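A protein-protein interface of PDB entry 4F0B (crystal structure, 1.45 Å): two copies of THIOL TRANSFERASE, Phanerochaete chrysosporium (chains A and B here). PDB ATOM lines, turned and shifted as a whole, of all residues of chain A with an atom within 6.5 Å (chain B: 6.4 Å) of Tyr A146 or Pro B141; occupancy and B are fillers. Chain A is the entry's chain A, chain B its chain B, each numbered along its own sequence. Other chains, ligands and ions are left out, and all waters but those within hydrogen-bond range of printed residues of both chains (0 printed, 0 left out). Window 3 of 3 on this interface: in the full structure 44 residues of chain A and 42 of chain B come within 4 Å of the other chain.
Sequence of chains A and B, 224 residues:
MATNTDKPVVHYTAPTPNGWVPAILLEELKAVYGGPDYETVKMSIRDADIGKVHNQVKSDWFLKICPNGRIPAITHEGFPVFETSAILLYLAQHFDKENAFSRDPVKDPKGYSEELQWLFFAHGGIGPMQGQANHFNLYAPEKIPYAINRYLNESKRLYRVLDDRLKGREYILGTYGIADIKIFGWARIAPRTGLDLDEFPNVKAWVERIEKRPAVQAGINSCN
A ring nitrogen (NE2) of His B135 sits at hydrogen-bond distance from the side-chain hydroxyl (OH) of Tyr A146 (2.7 Å).
ND1 of His B135 sits close to NH1 of Arg A150 (3.5 Å).
OH of Tyr A151 sits at hydrogen-bond distance from NE of Arg A150, at 3.3 Å.
The backbone carbonyl oxygen (O) of His B135 sits at hydrogen-bond distance from the backbone NH (N) of Ala B140 (3.0 Å).
Among the printed residues, pairs that only touch across the chains: Ile A144 with Ile B144 (3.9 Å), Tyr A146 with Phe B136 (3.8 Å), Tyr A146 with Ala B140 (3.6 Å), Tyr A146 with Pro B141 (3.5 Å), Tyr A146 with Ile B144 (3.7 Å) and Tyr A151 with Phe B136 (3.3 Å).
Tyr A146 touches just these residues of chain B: His B135, Phe B136, Ala B140, Pro B141 and Ile B144.
Of the printed residues of chain A, Pro B141 touches Tyr A146 (3.5 Å).
Of the printed residues of chain A, Phe B136 touches Tyr A146 (3.8 Å) and Tyr A151 (3.3 Å).
Printed residues of chain A within 4 Å of Ile B144: Ile A144 (3.9 Å) and Tyr A146 (3.7 Å).
Printed residues of chain A within 4 Å of His B135: Tyr A146 (2.7 Å) and Arg A150 (3.3 Å).
The nearest printed residue of chain A that does not touch Pro B141 is Arg A150 (7.9 Å).
The nearest printed residue of chain B that does not touch Ile A144 is Phe B136 (6.2 Å).
Of the 8 printed residues of chain A, 4 touch a printed residue of chain B.
Of the 8 printed residues of chain B, 5 touch a printed residue of chain A.
Ile A144 touches its own counterpart, Ile B144.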
ATOM      1  N   ILE A 144     -18.454  32.590  22.996  1.00  0.00           N
ATOM      2  CA  ILE A 144     -17.910  31.438  23.722  1.00  0.00           C
ATOM      3  C   ILE A 144     -17.229  30.511  22.708  1.00  0.00           C
ATOM      4  O   ILE A 144     -17.893  29.664  22.086  1.00  0.00           O
ATOM      5  CB  ILE A 144     -19.029  30.708  24.436  1.00  0.00           C
ATOM      6  CG1 ILE A 144     -19.801  31.716  25.307  1.00  0.00           C
ATOM      7  CG2 ILE A 144     -18.472  29.575  25.272  1.00  0.00           C
ATOM      8  CD1 ILE A 144     -21.002  31.154  25.969  1.00  0.00           C
ATOM      9  N   PRO A 145     -15.916  30.696  22.494  1.00  0.00           N
ATOM     10  CA  PRO A 145     -15.241  29.973  21.419  1.00  0.00           C
ATOM     11  C   PRO A 145     -15.394  28.458  21.530  1.00  0.00           C
ATOM     12  O   PRO A 145     -15.589  27.813  20.511  1.00  0.00           O
ATOM     13  CB  PRO A 145     -13.773  30.409  21.561  1.00  0.00           C
ATOM     14  CG  PRO A 145     -13.916  31.819  22.097  1.00  0.00           C
ATOM     15  CD  PRO A 145     -15.065  31.743  23.089  1.00  0.00           C
ATOM     16  N   TYR A 146     -15.355  27.895  22.731  1.00  0.00           N
ATOM     17  CA  TYR A 146     -15.523  26.445  22.835  1.00  0.00           C
ATOM     18  C   TYR A 146     -16.838  25.982  22.199  1.00  0.00           C
ATOM     19  O   TYR A 146     -16.884  24.961  21.505  1.00  0.00           O
ATOM     20  CB  TYR A 146     -15.459  25.975  24.315  1.00  0.00           C
ATOM     21  CG  TYR A 146     -15.789  24.509  24.431  1.00  0.00           C
ATOM     22  CD1 TYR A 146     -14.842  23.546  24.153  1.00  0.00           C
ATOM     23  CD2 TYR A 146     -17.089  24.081  24.745  1.00  0.00           C
ATOM     24  CE1 TYR A 146     -15.142  22.202  24.204  1.00  0.00           C
ATOM     25  CE2 TYR A 146     -17.425  22.743  24.791  1.00  0.00           C
ATOM     26  CZ  TYR A 146     -16.441  21.798  24.524  1.00  0.00           C
ATOM     27  OH  TYR A 146     -16.712  20.453  24.536  1.00  0.00           O
ATOM     28  N   ALA A 147     -17.921  26.695  22.496  1.00  0.00           N
ATOM     29  CA  ALA A 147     -19.222  26.311  21.994  1.00  0.00           C
ATOM     30  C   ALA A 147     -19.403  26.585  20.519  1.00  0.00           C
ATOM     31  O   ALA A 147     -19.967  25.746  19.810  1.00  0.00           O
ATOM     32  CB  ALA A 147     -20.313  27.019  22.798  1.00  0.00           C
ATOM     33  N   ILE A 148     -18.908  27.726  20.053  1.00  0.00           N
ATOM     34  CA  ILE A 148     -18.922  28.033  18.637  1.00  0.00           C
ATOM     35  C   ILE A 148     -18.196  26.897  17.880  1.00  0.00           C
ATOM     36  O   ILE A 148     -18.716  26.340  16.899  1.00  0.00           O
ATOM     37  CB  ILE A 148     -18.248  29.374  18.360  1.00  0.00           C
ATOM     38  CG1 ILE A 148     -19.094  30.521  18.957  1.00  0.00           C
ATOM     39  CG2 ILE A 148     -18.016  29.587  16.843  1.00  0.00           C
ATOM     40  CD1 ILE A 148     -18.383  31.899  18.961  1.00  0.00           C
ATOM     41  N   ASN A 149     -17.007  26.532  18.336  1.00  0.00           N
ATOM     42  CA  ASN A 149     -16.261  25.491  17.645  1.00  0.00           C
ATOM     43  C   ASN A 149     -16.942  24.129  17.750  1.00  0.00           C
ATOM     44  O   ASN A 149     -16.993  23.367  16.779  1.00  0.00           O
ATOM     45  CB  ASN A 149     -14.829  25.429  18.179  1.00  0.00           C
ATOM     46  CG  ASN A 149     -14.036  26.651  17.805  1.00  0.00           C
ATOM     47  OD1 ASN A 149     -14.347  27.318  16.825  1.00  0.00           O
ATOM     48  ND2 ASN A 149     -13.005  26.954  18.583  1.00  0.00           N
ATOM     49  N   ARG A 150     -17.465  23.796  18.924  1.00  0.00           N
ATOM     50  CA  ARG A 150     -18.127  22.491  19.058  1.00  0.00           C
ATOM     51  C   ARG A 150     -19.226  22.328  18.014  1.00  0.00           C
ATOM     52  O   ARG A 150     -19.324  21.303  17.320  1.00  0.00           O
ATOM     53  CB  ARG A 150     -18.732  22.318  20.459  1.00  0.00           C
ATOM     54  CG  ARG A 150     -19.754  21.198  20.522  1.00  0.00           C
ATOM     55  CD  ARG A 150     -20.056  20.821  21.996  1.00  0.00           C
ATOM     56  NE  ARG A 150     -21.175  19.894  22.109  1.00  0.00           N
ATOM     57  CZ  ARG A 150     -21.104  18.576  21.902  1.00  0.00           C
ATOM     58  NH1 ARG A 150     -19.941  17.982  21.581  1.00  0.00           N
ATOM     59  NH2 ARG A 150     -22.227  17.867  21.969  1.00  0.00           N
ATOM     60  N   TYR A 151     -20.088  23.341  17.910  1.00  0.00           N
ATOM     61  CA  TYR A 151     -21.249  23.190  17.021  1.00  0.00           C
ATOM     62  C   TYR A 151     -20.922  23.447  15.569  1.00  0.00           C
ATOM     63  O   TYR A 151     -21.552  22.816  14.721  1.00  0.00           O
ATOM     64  CB  TYR A 151     -22.479  23.993  17.535  1.00  0.00           C
ATOM     65  CG  TYR A 151     -22.916  23.443  18.867  1.00  0.00           C
ATOM     66  CD1 TYR A 151     -23.490  22.172  18.929  1.00  0.00           C
ATOM     67  CD2 TYR A 151     -22.676  24.140  20.052  1.00  0.00           C
ATOM     68  CE1 TYR A 151     -23.821  21.591  20.154  1.00  0.00           C
ATOM     69  CE2 TYR A 151     -23.013  23.592  21.285  1.00  0.00           C
ATOM     70  CZ  TYR A 151     -23.570  22.317  21.335  1.00  0.00           C
ATOM     71  OH  TYR A 151     -23.890  21.745  22.549  1.00  0.00           O
ATOM     72  N   HIS B 135     -23.650  17.152  27.919  1.00  0.00           N
ATOM     73  CA  HIS B 135     -22.348  17.538  27.395  1.00  0.00           C
ATOM     74  C   HIS B 135     -21.642  18.576  28.269  1.00  0.00           C
ATOM     75  O   HIS B 135     -20.448  18.410  28.616  1.00  0.00           O
ATOM     76  CB  HIS B 135     -22.428  18.102  25.978  1.00  0.00           C
ATOM     77  CG  HIS B 135     -21.072  18.508  25.484  1.00  0.00           C
ATOM     78  ND1 HIS B 135     -20.173  17.566  25.025  1.00  0.00           N
ATOM     79  CD2 HIS B 135     -20.413  19.697  25.495  1.00  0.00           C
ATOM     80  CE1 HIS B 135     -19.021  18.168  24.750  1.00  0.00           C
ATOM     81  NE2 HIS B 135     -19.141  19.456  25.016  1.00  0.00           N
ATOM     82  N   PHE B 136     -22.354  19.651  28.616  1.00  0.00           N
ATOM     83  CA  PHE B 136     -21.732  20.727  29.358  1.00  0.00           C
ATOM     84  C   PHE B 136     -21.484  20.396  30.841  1.00  0.00           C
ATOM     85  O   PHE B 136     -20.738  21.129  31.494  1.00  0.00           O
ATOM     86  CB  PHE B 136     -22.467  22.056  29.113  1.00  0.00           C
ATOM     87  CG  PHE B 136     -22.155  22.637  27.764  1.00  0.00           C
ATOM     88  CD1 PHE B 136     -20.978  23.355  27.576  1.00  0.00           C
ATOM     89  CD2 PHE B 136     -22.990  22.414  26.672  1.00  0.00           C
ATOM     90  CE1 PHE B 136     -20.649  23.893  26.338  1.00  0.00           C
ATOM     91  CE2 PHE B 136     -22.681  22.939  25.433  1.00  0.00           C
ATOM     92  CZ  PHE B 136     -21.520  23.678  25.255  1.00  0.00           C
ATOM     93  N   TYR B 139     -18.587  16.497  29.647  1.00  0.00           N
ATOM     94  CA  TYR B 139     -17.539  16.386  28.620  1.00  0.00           C
ATOM     95  C   TYR B 139     -16.839  17.689  28.279  1.00  0.00           C
ATOM     96  O   TYR B 139     -15.661  17.666  27.915  1.00  0.00           O
ATOM     97  CB  TYR B 139     -18.100  15.712  27.375  1.00  0.00           C
ATOM     98  CG  TYR B 139     -18.822  14.402  27.694  1.00  0.00           C
ATOM     99  CD1 TYR B 139     -18.111  13.284  28.051  1.00  0.00           C
ATOM    100  CD2 TYR B 139     -20.210  14.303  27.642  1.00  0.00           C
ATOM    101  CE1 TYR B 139     -18.748  12.093  28.369  1.00  0.00           C
ATOM    102  CE2 TYR B 139     -20.858  13.119  27.953  1.00  0.00           C
ATOM    103  CZ  TYR B 139     -20.116  12.015  28.315  1.00  0.00           C
ATOM    104  OH  TYR B 139     -20.764  10.831  28.620  1.00  0.00           O
ATOM    105  N   ALA B 140     -17.531  18.823  28.370  1.00  0.00           N
ATOM    106  CA  ALA B 140     -16.865  20.087  28.113  1.00  0.00           C
ATOM    107  C   ALA B 140     -15.709  20.245  29.106  1.00  0.00           C
ATOM    108  O   ALA B 140     -15.896  20.023  30.302  1.00  0.00           O
ATOM    109  CB  ALA B 140     -17.849  21.243  28.278  1.00  0.00           C
ATOM    110  N   PRO B 141     -14.507  20.612  28.654  1.00  0.00           N
ATOM    111  CA  PRO B 141     -13.380  20.706  29.580  1.00  0.00           C
ATOM    112  C   PRO B 141     -13.504  21.827  30.608  1.00  0.00           C
ATOM    113  O   PRO B 141     -12.864  21.733  31.675  1.00  0.00           O
ATOM    114  CB  PRO B 141     -12.169  20.974  28.651  1.00  0.00           C
ATOM    115  CG  PRO B 141     -12.615  20.649  27.265  1.00  0.00           C
ATOM    116  CD  PRO B 141     -14.119  20.670  27.233  1.00  0.00           C
ATOM    117  N   GLU B 142     -14.240  22.886  30.299  1.00  0.00           N
ATOM    118  CA  GLU B 142     -14.418  23.987  31.229  1.00  0.00           C
ATOM    119  C   GLU B 142     -15.870  24.098  31.624  1.00  0.00           C
ATOM    120  O   GLU B 142     -16.761  23.700  30.872  1.00  0.00           O
ATOM    121  CB  GLU B 142     -14.001  25.302  30.611  1.00  0.00           C
ATOM    122  CG  GLU B 142     -12.499  25.367  30.379  1.00  0.00           C
ATOM    123  CD  GLU B 142     -12.077  26.736  29.946  1.00  0.00           C
ATOM    124  OE1 GLU B 142     -12.095  26.998  28.721  1.00  0.00           O
ATOM    125  OE2 GLU B 142     -11.750  27.555  30.835  1.00  0.00           O
ATOM    126  N   LYS B 143     -16.092  24.632  32.821  1.00  0.00           N
ATOM    127  CA  LYS B 143     -17.432  25.015  33.276  1.00  0.00           C
ATOM    128  C   LYS B 143     -17.824  26.303  32.553  1.00  0.00           C
ATOM    129  O   LYS B 143     -17.141  27.324  32.663  1.00  0.00           O
ATOM    130  CB  LYS B 143     -17.398  25.263  34.784  1.00  0.00           C
ATOM    131  CG  LYS B 143     -18.745  25.662  35.372  1.00  0.00           C
ATOM    132  CD  LYS B 143     -18.623  26.034  36.858  1.00  0.00           C
ATOM    133  CE  LYS B 143     -19.948  26.531  37.418  1.00  0.00           C
ATOM    134  NZ  LYS B 143     -19.875  26.729  38.883  1.00  0.00           N
ATOM    135  N   ILE B 144     -18.942  26.216  31.825  1.00  0.00           N
ATOM    136  CA  ILE B 144     -19.422  27.345  31.004  1.00  0.00           C
ATOM    137  C   ILE B 144     -20.862  27.643  31.440  1.00  0.00           C
ATOM    138  O   ILE B 144     -21.814  27.064  30.904  1.00  0.00           O
ATOM    139  CB  ILE B 144     -19.332  27.051  29.503  1.00  0.00           C
ATOM    140  CG1 ILE B 144     -17.899  26.672  29.110  1.00  0.00           C
ATOM    141  CG2 ILE B 144     -19.834  28.264  28.679  1.00  0.00           C
ATOM    142  CD1 ILE B 144     -17.784  26.207  27.682  1.00  0.00           C
